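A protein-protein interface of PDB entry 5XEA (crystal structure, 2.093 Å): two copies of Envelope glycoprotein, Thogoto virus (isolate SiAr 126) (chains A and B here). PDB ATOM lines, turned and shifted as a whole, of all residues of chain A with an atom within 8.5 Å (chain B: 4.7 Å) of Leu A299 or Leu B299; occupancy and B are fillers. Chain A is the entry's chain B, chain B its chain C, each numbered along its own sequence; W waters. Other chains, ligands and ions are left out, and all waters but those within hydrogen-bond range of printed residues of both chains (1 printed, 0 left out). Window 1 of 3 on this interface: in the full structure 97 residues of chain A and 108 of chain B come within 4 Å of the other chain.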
ATOM      1  N   GLN A 292      24.606   5.625 -26.513  1.00  0.00           N
ATOM      2  CA  GLN A 292      25.248   4.466 -25.902  1.00  0.00           C
ATOM      3  C   GLN A 292      24.947   4.389 -24.408  1.00  0.00           C
ATOM      4  O   GLN A 292      24.566   3.329 -23.891  1.00  0.00           O
ATOM      5  CB  GLN A 292      26.758   4.530 -26.149  1.00  0.00           C
ATOM      6  CG  GLN A 292      27.544   3.317 -25.644  1.00  0.00           C
ATOM      7  CD  GLN A 292      29.067   3.484 -25.754  1.00  0.00           C
ATOM      8  OE1 GLN A 292      29.718   2.835 -26.581  1.00  0.00           O
ATOM      9  NE2 GLN A 292      29.638   4.343 -24.907  1.00  0.00           N
ATOM     10  N   ALA A 293      25.081   5.519 -23.702  1.00  0.00           N
ATOM     11  CA  ALA A 293      24.864   5.523 -22.256  1.00  0.00           C
ATOM     12  C   ALA A 293      23.428   5.156 -21.910  1.00  0.00           C
ATOM     13  O   ALA A 293      23.180   4.421 -20.947  1.00  0.00           O
ATOM     14  CB  ALA A 293      25.212   6.895 -21.665  1.00  0.00           C
ATOM     15  N   PHE A 294      22.465   5.706 -22.652  1.00  0.00           N
ATOM     16  CA  PHE A 294      21.070   5.416 -22.360  1.00  0.00           C
ATOM     17  C   PHE A 294      20.782   3.938 -22.572  1.00  0.00           C
ATOM     18  O   PHE A 294      20.142   3.291 -21.735  1.00  0.00           O
ATOM     19  CB  PHE A 294      20.151   6.275 -23.230  1.00  0.00           C
ATOM     20  CG  PHE A 294      18.706   5.928 -23.085  1.00  0.00           C
ATOM     21  CD1 PHE A 294      17.946   6.491 -22.068  1.00  0.00           C
ATOM     22  CD2 PHE A 294      18.104   5.011 -23.938  1.00  0.00           C
ATOM     23  CE1 PHE A 294      16.605   6.142 -21.908  1.00  0.00           C
ATOM     24  CE2 PHE A 294      16.756   4.663 -23.779  1.00  0.00           C
ATOM     25  CZ  PHE A 294      16.016   5.240 -22.767  1.00  0.00           C
ATOM     26  N   GLU A 295      21.275   3.377 -23.683  1.00  0.00           N
ATOM     27  CA  GLU A 295      21.043   1.963 -23.957  1.00  0.00           C
ATOM     28  C   GLU A 295      21.720   1.080 -22.914  1.00  0.00           C
ATOM     29  O   GLU A 295      21.153   0.064 -22.490  1.00  0.00           O
ATOM     30  CB  GLU A 295      21.521   1.617 -25.363  1.00  0.00           C
ATOM     31  CG  GLU A 295      20.786   2.389 -26.459  1.00  0.00           C
ATOM     32  CD  GLU A 295      19.325   1.988 -26.622  1.00  0.00           C
ATOM     33  OE1 GLU A 295      19.007   0.789 -26.499  1.00  0.00           O
ATOM     34  OE2 GLU A 295      18.484   2.869 -26.898  1.00  0.00           O
ATOM     35  N   LEU A 296      22.923   1.454 -22.471  1.00  0.00           N
ATOM     36  CA  LEU A 296      23.620   0.621 -21.496  1.00  0.00           C
ATOM     37  C   LEU A 296      22.959   0.668 -20.118  1.00  0.00           C
ATOM     38  O   LEU A 296      22.941  -0.348 -19.408  1.00  0.00           O
ATOM     39  CB  LEU A 296      25.087   1.026 -21.398  1.00  0.00           C
ATOM     40  CG  LEU A 296      25.964   0.707 -22.622  1.00  0.00           C
ATOM     41  CD1 LEU A 296      27.288   1.494 -22.570  1.00  0.00           C
ATOM     42  CD2 LEU A 296      26.232  -0.783 -22.751  1.00  0.00           C
ATOM     43  N   GLU A 297      22.404   1.818 -19.725  1.00  0.00           N
ATOM     44  CA  GLU A 297      21.674   1.860 -18.461  1.00  0.00           C
ATOM     45  C   GLU A 297      20.329   1.137 -18.572  1.00  0.00           C
ATOM     46  O   GLU A 297      19.823   0.607 -17.573  1.00  0.00           O
ATOM     47  CB  GLU A 297      21.485   3.306 -17.995  1.00  0.00           C
ATOM     48  CG  GLU A 297      22.803   4.060 -17.701  1.00  0.00           C
ATOM     49  CD  GLU A 297      23.495   3.584 -16.434  1.00  0.00           C
ATOM     50  OE1 GLU A 297      22.804   3.395 -15.417  1.00  0.00           O
ATOM     51  OE2 GLU A 297      24.726   3.381 -16.447  1.00  0.00           O
ATOM     52  N   GLY A 298      19.742   1.104 -19.770  1.00  0.00           N
ATOM     53  CA  GLY A 298      18.579   0.264 -19.991  1.00  0.00           C
ATOM     54  C   GLY A 298      18.914  -1.215 -19.906  1.00  0.00           C
ATOM     55  O   GLY A 298      18.176  -1.998 -19.297  1.00  0.00           O
ATOM     56  N   LEU A 299      20.039  -1.620 -20.506  1.00  0.00           N
ATOM     57  CA  LEU A 299      20.460  -3.013 -20.387  1.00  0.00           C
ATOM     58  C   LEU A 299      20.763  -3.367 -18.939  1.00  0.00           C
ATOM     59  O   LEU A 299      20.501  -4.494 -18.504  1.00  0.00           O
ATOM     60  CB  LEU A 299      21.671  -3.289 -21.284  1.00  0.00           C
ATOM     61  CG  LEU A 299      21.371  -3.283 -22.786  1.00  0.00           C
ATOM     62  CD1 LEU A 299      22.668  -3.162 -23.586  1.00  0.00           C
ATOM     63  CD2 LEU A 299      20.578  -4.551 -23.193  1.00  0.00           C
ATOM     64  N   ARG A 300      21.304  -2.411 -18.176  1.00  0.00           N
ATOM     65  CA  ARG A 300      21.530  -2.623 -16.750  1.00  0.00           C
ATOM     66  C   ARG A 300      20.220  -2.907 -16.021  1.00  0.00           C
ATOM     67  O   ARG A 300      20.117  -3.875 -15.257  1.00  0.00           O
ATOM     68  CB  ARG A 300      22.222  -1.401 -16.145  1.00  0.00           C
ATOM     69  CG  ARG A 300      22.656  -1.591 -14.685  1.00  0.00           C
ATOM     70  CD  ARG A 300      23.320  -0.308 -14.123  1.00  0.00           C
ATOM     71  NE  ARG A 300      23.981  -0.515 -12.837  1.00  0.00           N
ATOM     72  CZ  ARG A 300      25.186  -1.057 -12.689  1.00  0.00           C
ATOM     73  NH1 ARG A 300      25.880  -1.451 -13.744  1.00  0.00           N
ATOM     74  NH2 ARG A 300      25.699  -1.221 -11.482  1.00  0.00           N
ATOM     75  N   ALA A 301      19.206  -2.060 -16.241  1.00  0.00           N
ATOM     76  CA  ALA A 301      17.905  -2.265 -15.617  1.00  0.00           C
ATOM     77  C   ALA A 301      17.287  -3.597 -16.038  1.00  0.00           C
ATOM     78  O   ALA A 301      16.657  -4.287 -15.227  1.00  0.00           O
ATOM     79  CB  ALA A 301      16.969  -1.115 -15.977  1.00  0.00           C
ATOM     80  N   SER A 302      17.447  -3.956 -17.312  1.00  0.00           N
ATOM     81  CA  SER A 302      16.868  -5.182 -17.824  1.00  0.00           C
ATOM     82  C   SER A 302      17.589  -6.401 -17.266  1.00  0.00           C
ATOM     83  O   SER A 302      16.947  -7.410 -16.939  1.00  0.00           O
ATOM     84  CB  SER A 302      16.905  -5.167 -19.348  1.00  0.00           C
ATOM     85  OG  SER A 302      15.740  -4.534 -19.866  1.00  0.00           O
ATOM     86  N   PHE A 303      18.916  -6.326 -17.138  1.00  0.00           N
ATOM     87  CA  PHE A 303      19.643  -7.385 -16.448  1.00  0.00           C
ATOM     88  C   PHE A 303      19.162  -7.547 -15.009  1.00  0.00           C
ATOM     89  O   PHE A 303      19.033  -8.674 -14.522  1.00  0.00           O
ATOM     90  CB  PHE A 303      21.142  -7.123 -16.485  1.00  0.00           C
ATOM     91  CG  PHE A 303      21.789  -7.602 -17.736  1.00  0.00           C
ATOM     92  CD1 PHE A 303      21.043  -7.745 -18.887  1.00  0.00           C
ATOM     93  CD2 PHE A 303      23.132  -7.922 -17.768  1.00  0.00           C
ATOM     94  CE1 PHE A 303      21.618  -8.204 -20.059  1.00  0.00           C
ATOM     95  CE2 PHE A 303      23.723  -8.380 -18.942  1.00  0.00           C
ATOM     96  CZ  PHE A 303      22.958  -8.527 -20.088  1.00  0.00           C
ATOM     97  N   ALA A 304      18.873  -6.439 -14.323  1.00  0.00           N
ATOM     98  CA  ALA A 304      18.333  -6.528 -12.969  1.00  0.00           C
ATOM     99  C   ALA A 304      16.994  -7.262 -12.947  1.00  0.00           C
ATOM    100  O   ALA A 304      16.710  -8.003 -12.001  1.00  0.00           O
ATOM    101  CB  ALA A 304      18.185  -5.139 -12.356  1.00  0.00           C
ATOM    102  N   GLU A 305      16.155  -7.073 -13.973  1.00  0.00           N
ATOM    103  CA  GLU A 305      14.891  -7.807 -14.008  1.00  0.00           C
ATOM    104  C   GLU A 305      15.132  -9.291 -14.276  1.00  0.00           C
ATOM    105  O   GLU A 305      14.445 -10.148 -13.707  1.00  0.00           O
ATOM    106  CB  GLU A 305      13.941  -7.199 -15.055  1.00  0.00           C
ATOM    107  CG  GLU A 305      12.673  -8.030 -15.383  1.00  0.00           C
ATOM    108  CD  GLU A 305      11.759  -8.280 -14.174  1.00  0.00           C
ATOM    109  OE1 GLU A 305      11.803  -7.487 -13.208  1.00  0.00           O
ATOM    110  OE2 GLU A 305      10.999  -9.279 -14.177  1.00  0.00           O
ATOM    111  N   LEU A 306      16.116  -9.610 -15.124  1.00  0.00           N
ATOM    112  CA  LEU A 306      16.462 -11.006 -15.386  1.00  0.00           C
ATOM    113  C   LEU A 306      16.922 -11.715 -14.117  1.00  0.00           C
ATOM    114  O   LEU A 306      16.494 -12.844 -13.838  1.00  0.00           O
ATOM    115  CB  LEU A 306      17.543 -11.093 -16.464  1.00  0.00           C
ATOM    116  CG  LEU A 306      17.062 -10.661 -17.847  1.00  0.00           C
ATOM    117  CD1 LEU A 306      18.190 -10.747 -18.880  1.00  0.00           C
ATOM    118  CD2 LEU A 306      15.858 -11.503 -18.270  1.00  0.00           C
ATOM    119  N   LEU A 403      20.453 -18.291 -28.544  1.00  0.00           N
ATOM    120  CA  LEU A 403      20.649 -16.859 -28.375  1.00  0.00           C
ATOM    121  C   LEU A 403      21.637 -16.344 -29.405  1.00  0.00           C
ATOM    122  O   LEU A 403      22.625 -17.006 -29.724  1.00  0.00           O
ATOM    123  CB  LEU A 403      21.192 -16.540 -26.986  1.00  0.00           C
ATOM    124  CG  LEU A 403      20.239 -16.525 -25.803  1.00  0.00           C
ATOM    125  CD1 LEU A 403      21.025 -16.089 -24.552  1.00  0.00           C
ATOM    126  CD2 LEU A 403      19.113 -15.567 -26.130  1.00  0.00           C
ATOM    127  N   TRP A 404      21.373 -15.160 -29.928  1.00  0.00           N
ATOM    128  CA  TRP A 404      22.427 -14.414 -30.592  1.00  0.00           C
ATOM    129  C   TRP A 404      23.236 -13.693 -29.527  1.00  0.00           C
ATOM    130  O   TRP A 404      22.672 -13.077 -28.618  1.00  0.00           O
ATOM    131  CB  TRP A 404      21.852 -13.433 -31.604  1.00  0.00           C
ATOM    132  CG  TRP A 404      22.875 -12.527 -32.208  1.00  0.00           C
ATOM    133  CD1 TRP A 404      23.609 -12.746 -33.344  1.00  0.00           C
ATOM    134  CD2 TRP A 404      23.273 -11.245 -31.711  1.00  0.00           C
ATOM    135  NE1 TRP A 404      24.443 -11.681 -33.576  1.00  0.00           N
ATOM    136  CE2 TRP A 404      24.256 -10.744 -32.594  1.00  0.00           C
ATOM    137  CE3 TRP A 404      22.897 -10.474 -30.606  1.00  0.00           C
ATOM    138  CZ2 TRP A 404      24.860  -9.502 -32.412  1.00  0.00           C
ATOM    139  CZ3 TRP A 404      23.502  -9.238 -30.421  1.00  0.00           C
ATOM    140  CH2 TRP A 404      24.475  -8.768 -31.322  1.00  0.00           C
ATOM    141  N   TYR A 405      24.559 -13.821 -29.611  1.00  0.00           N
ATOM    142  CA  TYR A 405      25.507 -13.250 -28.681  1.00  0.00           C
ATOM    143  C   TYR A 405      26.151 -12.021 -29.310  1.00  0.00           C
ATOM    144  O   TYR A 405      26.556 -12.070 -30.480  1.00  0.00           O
ATOM    145  CB  TYR A 405      26.593 -14.260 -28.326  1.00  0.00           C
ATOM    146  CG  TYR A 405      26.203 -15.304 -27.297  1.00  0.00           C
ATOM    147  CD1 TYR A 405      26.762 -15.299 -26.027  1.00  0.00           C
ATOM    148  CD2 TYR A 405      25.294 -16.308 -27.606  1.00  0.00           C
ATOM    149  CE1 TYR A 405      26.413 -16.267 -25.090  1.00  0.00           C
ATOM    150  CE2 TYR A 405      24.942 -17.265 -26.667  1.00  0.00           C
ATOM    151  CZ  TYR A 405      25.505 -17.238 -25.424  1.00  0.00           C
ATOM    152  OH  TYR A 405      25.149 -18.205 -24.510  1.00  0.00           O
ATOM    153  N   PRO A 406      26.278 -10.922 -28.585  1.00  0.00           N
ATOM    154  CA  PRO A 406      27.001  -9.763 -29.124  1.00  0.00           C
ATOM    155  C   PRO A 406      28.498 -10.020 -29.170  1.00  0.00           C
ATOM    156  O   PRO A 406      29.024 -10.987 -28.612  1.00  0.00           O
ATOM    157  CB  PRO A 406      26.663  -8.641 -28.145  1.00  0.00           C
ATOM    158  CG  PRO A 406      26.383  -9.348 -26.861  1.00  0.00           C
ATOM    159  CD  PRO A 406      25.725 -10.659 -27.246  1.00  0.00           C
ATOM    160  N   SER A 407      29.188  -9.110 -29.848  1.00  0.00           N
ATOM    161  CA  SER A 407      30.622  -9.215 -30.048  1.00  0.00           C
ATOM    162  C   SER A 407      31.155  -7.817 -30.338  1.00  0.00           C
ATOM    163  O   SER A 407      30.466  -6.988 -30.933  1.00  0.00           O
ATOM    164  CB  SER A 407      30.966 -10.163 -31.205  1.00  0.00           C
ATOM    165  OG  SER A 407      32.357 -10.405 -31.288  1.00  0.00           O
ATOM    166  N   GLU B 295      32.013  -3.143 -23.564  1.00  0.00           N
ATOM    167  CA  GLU B 295      30.650  -3.397 -23.128  1.00  0.00           C
ATOM    168  C   GLU B 295      30.053  -4.596 -23.860  1.00  0.00           C
ATOM    169  O   GLU B 295      29.446  -5.475 -23.233  1.00  0.00           O
ATOM    170  CB  GLU B 295      29.801  -2.146 -23.329  1.00  0.00           C
ATOM    171  CG  GLU B 295      30.235  -0.974 -22.446  1.00  0.00           C
ATOM    172  CD  GLU B 295      30.137  -1.288 -20.954  1.00  0.00           C
ATOM    173  OE1 GLU B 295      29.053  -1.713 -20.485  1.00  0.00           O
ATOM    174  OE2 GLU B 295      31.151  -1.124 -20.242  1.00  0.00           O
ATOM    175  N   LEU B 296      30.251  -4.672 -25.182  1.00  0.00           N
ATOM    176  CA  LEU B 296      29.679  -5.775 -25.950  1.00  0.00           C
ATOM    177  C   LEU B 296      30.264  -7.119 -25.526  1.00  0.00           C
ATOM    178  O   LEU B 296      29.555  -8.126 -25.516  1.00  0.00           O
ATOM    179  CB  LEU B 296      29.885  -5.545 -27.446  1.00  0.00           C
ATOM    180  CG  LEU B 296      29.060  -4.443 -28.129  1.00  0.00           C
ATOM    181  CD1 LEU B 296      29.659  -4.048 -29.487  1.00  0.00           C
ATOM    182  CD2 LEU B 296      27.607  -4.845 -28.291  1.00  0.00           C
ATOM    183  N   GLU B 297      31.553  -7.156 -25.174  1.00  0.00           N
ATOM    184  CA  GLU B 297      32.165  -8.403 -24.723  1.00  0.00           C
ATOM    185  C   GLU B 297      31.670  -8.793 -23.333  1.00  0.00           C
ATOM    186  O   GLU B 297      31.481  -9.982 -23.043  1.00  0.00           O
ATOM    187  CB  GLU B 297      33.682  -8.276 -24.747  1.00  0.00           C
ATOM    188  CG  GLU B 297      34.231  -8.234 -26.156  1.00  0.00           C
ATOM    189  CD  GLU B 297      34.215  -9.596 -26.827  1.00  0.00           C
ATOM    190  OE1 GLU B 297      34.519 -10.589 -26.125  1.00  0.00           O
ATOM    191  OE2 GLU B 297      33.900  -9.671 -28.042  1.00  0.00           O
ATOM    192  N   GLY B 298      31.458  -7.810 -22.465  1.00  0.00           N
ATOM    193  CA  GLY B 298      30.851  -8.105 -21.181  1.00  0.00           C
ATOM    194  C   GLY B 298      29.453  -8.674 -21.329  1.00  0.00           C
ATOM    195  O   GLY B 298      29.101  -9.654 -20.672  1.00  0.00           O
ATOM    196  N   LEU B 299      28.647  -8.073 -22.211  1.00  0.00           N
ATOM    197  CA  LEU B 299      27.319  -8.597 -22.492  1.00  0.00           C
ATOM    198  C   LEU B 299      27.405 -10.022 -23.018  1.00  0.00           C
ATOM    199  O   LEU B 299      26.603 -10.888 -22.635  1.00  0.00           O
ATOM    200  CB  LEU B 299      26.605  -7.688 -23.491  1.00  0.00           C
ATOM    201  CG  LEU B 299      26.253  -6.292 -22.970  1.00  0.00           C
ATOM    202  CD1 LEU B 299      25.776  -5.398 -24.100  1.00  0.00           C
ATOM    203  CD2 LEU B 299      25.173  -6.366 -21.884  1.00  0.00           C
ATOM    204  N   ARG B 300      28.385 -10.282 -23.889  1.00  0.00           N
ATOM    205  CA  ARG B 300      28.635 -11.640 -24.355  1.00  0.00           C
ATOM    206  C   ARG B 300      28.855 -12.599 -23.187  1.00  0.00           C
ATOM    207  O   ARG B 300      28.292 -13.702 -23.167  1.00  0.00           O
ATOM    208  CB  ARG B 300      29.843 -11.652 -25.279  1.00  0.00           C
ATOM    209  CG  ARG B 300      30.040 -12.950 -26.010  1.00  0.00           C
ATOM    210  CD  ARG B 300      31.202 -12.829 -26.971  1.00  0.00           C
ATOM    211  NE  ARG B 300      31.420 -14.070 -27.694  1.00  0.00           N
ATOM    212  CZ  ARG B 300      30.800 -14.382 -28.822  1.00  0.00           C
ATOM    213  NH1 ARG B 300      29.924 -13.540 -29.350  1.00  0.00           N
ATOM    214  NH2 ARG B 300      31.053 -15.538 -29.412  1.00  0.00           N
ATOM    215  N   ALA B 301      29.687 -12.204 -22.217  1.00  0.00           N
ATOM    216  CA  ALA B 301      29.945 -13.058 -21.062  1.00  0.00           C
ATOM    217  C   ALA B 301      28.678 -13.238 -20.241  1.00  0.00           C
ATOM    218  O   ALA B 301      28.392 -14.336 -19.741  1.00  0.00           O
ATOM    219  CB  ALA B 301      31.065 -12.466 -20.201  1.00  0.00           C
ATOM    220  N   SER B 302      27.878 -12.181 -20.137  1.00  0.00           N
ATOM    221  CA  SER B 302      26.650 -12.270 -19.364  1.00  0.00           C
ATOM    222  C   SER B 302      25.595 -13.105 -20.080  1.00  0.00           C
ATOM    223  O   SER B 302      24.818 -13.815 -19.431  1.00  0.00           O
ATOM    224  CB  SER B 302      26.139 -10.868 -19.062  1.00  0.00           C
ATOM    225  OG  SER B 302      26.851 -10.370 -17.961  1.00  0.00           O
ATOM    226  N   PHE B 303      25.533 -13.019 -21.415  1.00  0.00           N
ATOM    227  CA  PHE B 303      24.652 -13.901 -22.172  1.00  0.00           C
ATOM    228  C   PHE B 303      25.047 -15.351 -21.993  1.00  0.00           C
ATOM    229  O   PHE B 303      24.179 -16.226 -21.891  1.00  0.00           O
ATOM    230  CB  PHE B 303      24.644 -13.543 -23.655  1.00  0.00           C
ATOM    231  CG  PHE B 303      23.659 -12.490 -23.998  1.00  0.00           C
ATOM    232  CD1 PHE B 303      23.329 -11.509 -23.067  1.00  0.00           C
ATOM    233  CD2 PHE B 303      23.045 -12.474 -25.231  1.00  0.00           C
ATOM    234  CE1 PHE B 303      22.404 -10.524 -23.361  1.00  0.00           C
ATOM    235  CE2 PHE B 303      22.115 -11.485 -25.539  1.00  0.00           C
ATOM    236  CZ  PHE B 303      21.788 -10.510 -24.594  1.00  0.00           C
ATOM    237  N   TRP B 404      12.573  -3.941 -20.460  1.00  0.00           N
ATOM    238  CA  TRP B 404      12.875  -2.889 -21.405  1.00  0.00           C
ATOM    239  C   TRP B 404      13.725  -3.484 -22.527  1.00  0.00           C
ATOM    240  O   TRP B 404      14.684  -4.214 -22.267  1.00  0.00           O
ATOM    241  CB  TRP B 404      13.591  -1.734 -20.710  1.00  0.00           C
ATOM    242  CG  TRP B 404      14.036  -0.711 -21.670  1.00  0.00           C
ATOM    243  CD1 TRP B 404      13.315   0.339 -22.154  1.00  0.00           C
ATOM    244  CD2 TRP B 404      15.305  -0.662 -22.303  1.00  0.00           C
ATOM    245  NE1 TRP B 404      14.069   1.045 -23.048  1.00  0.00           N
ATOM    246  CE2 TRP B 404      15.299   0.451 -23.158  1.00  0.00           C
ATOM    247  CE3 TRP B 404      16.451  -1.456 -22.233  1.00  0.00           C
ATOM    248  CZ2 TRP B 404      16.392   0.803 -23.931  1.00  0.00           C
ATOM    249  CZ3 TRP B 404      17.549  -1.100 -23.002  1.00  0.00           C
ATOM    250  CH2 TRP B 404      17.507   0.019 -23.843  1.00  0.00           C
ATOM    251  N   PRO B 406      16.211  -2.948 -25.884  1.00  0.00           N
ATOM    252  CA  PRO B 406      17.004  -1.985 -26.650  1.00  0.00           C
ATOM    253  C   PRO B 406      16.543  -1.939 -28.096  1.00  0.00           C
ATOM    254  O   PRO B 406      15.783  -2.787 -28.571  1.00  0.00           O
ATOM    255  CB  PRO B 406      18.429  -2.529 -26.538  1.00  0.00           C
ATOM    256  CG  PRO B 406      18.203  -4.016 -26.502  1.00  0.00           C
ATOM    257  CD  PRO B 406      16.975  -4.184 -25.622  1.00  0.00           C
HETATM  258  O   HOH W   1      33.636 -12.860 -29.888  1.00  0.00           O
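NH1 of Arg B300 lies within hydrogen-bond range of O of Pro A406, at 2.8 Å. The backbone carbonyl oxygen (O) of Phe B303 sits at hydrogen-bond distance from the side-chain hydroxyl (OH) of Tyr A405 (3.4 Å). The backbone carbonyl oxygen of Trp B404 sits at hydrogen-bond distance from the side-chain hydroxyl of Ser A302.
CZ2 of Trp B404 touches CE2 of Phe A294 (3.9 Å). Glu A295 touches Pro B406 (OE1 to CB, 3.4 Å). Leu A296 touches Glu B295. Leu A299 touches Trp B404. Phe A303 touches Phe B303 (CZ to CE1, 3.9 Å). Trp A404 touches Phe B303 (O to CD2, 3.5 Å). Tyr A405 touches Arg B300 (CB to NH1, 3.6 Å). Pro A406 touches Leu B299. CD of Pro A406 touches CD2 of Phe B303 (3.8 Å). Ser A407 touches Glu B297 (OG to OE2, 3.7 Å).
Glu A305 touches none of the printed residues of chain B. Leu A306 touches none of the printed residues of chain B. Of the printed residues of chain B, Trp A404 touches Phe B303. No residue of chain A comes within 4 Å of Gly B298. Of chain A, only Leu A299, Phe A303 and Pro A406 come within 4 Å of Leu B299. Printed residues of chain A within 4 Å of Pro B406: Glu A295 (3.4 Å). The nearest residue of chain A that does not touch Leu B299 is Leu A296 (4.8 Å). The nearest printed residue of chain A that does not touch Ser B302 is Tyr A405 (6.0 Å).
Of the 20 printed residues of chain A, 11 touch a printed residue of chain B. Printed residues of chain A that touch a printed residue of chain B: Phe A294, Glu A295, Leu A296, Gly A298, Leu A299, Ser A302, Phe A303, Trp A404, Tyr A405, Pro A406 and Ser A407. Of the 11 printed residues of chain B, 9 touch a printed residue of chain A. Printed residues of chain B that touch a printed residue of chain A: Glu B295, Leu B296, Glu B297, Leu B299, Arg B300, Ser B302, Phe B303, Trp B404 and Pro B406. Along chain B the printed residues that touch a printed residue of chain A span positions 295 to 406. Among the printed residues, no Asp or Glu carboxylate lies within 4 Å of a Lys or Arg side-chain nitrogen of the other chain.
Leu A296 touches Glu B295, but with the chains exchanged Glu A295 does not touch Leu B296 (9.3 Å). Ser A302 touches Trp B404, but with the chains exchanged Trp A404 does not touch Ser B302 (9.0 Å). Phe B303 touches its own counterpart, Phe A303. Trp A404 touches Phe B303, but with the chains exchanged Phe A303 does not touch Trp B404 (7.0 Å). Positions printed for both chains: 295, 296, 297, 298, 299, 300, 301, 302, 303, 404 and 406.
Water W1 bridges the side-chain hydroxyl of Ser A407 and the guanidinium group of Arg B300.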
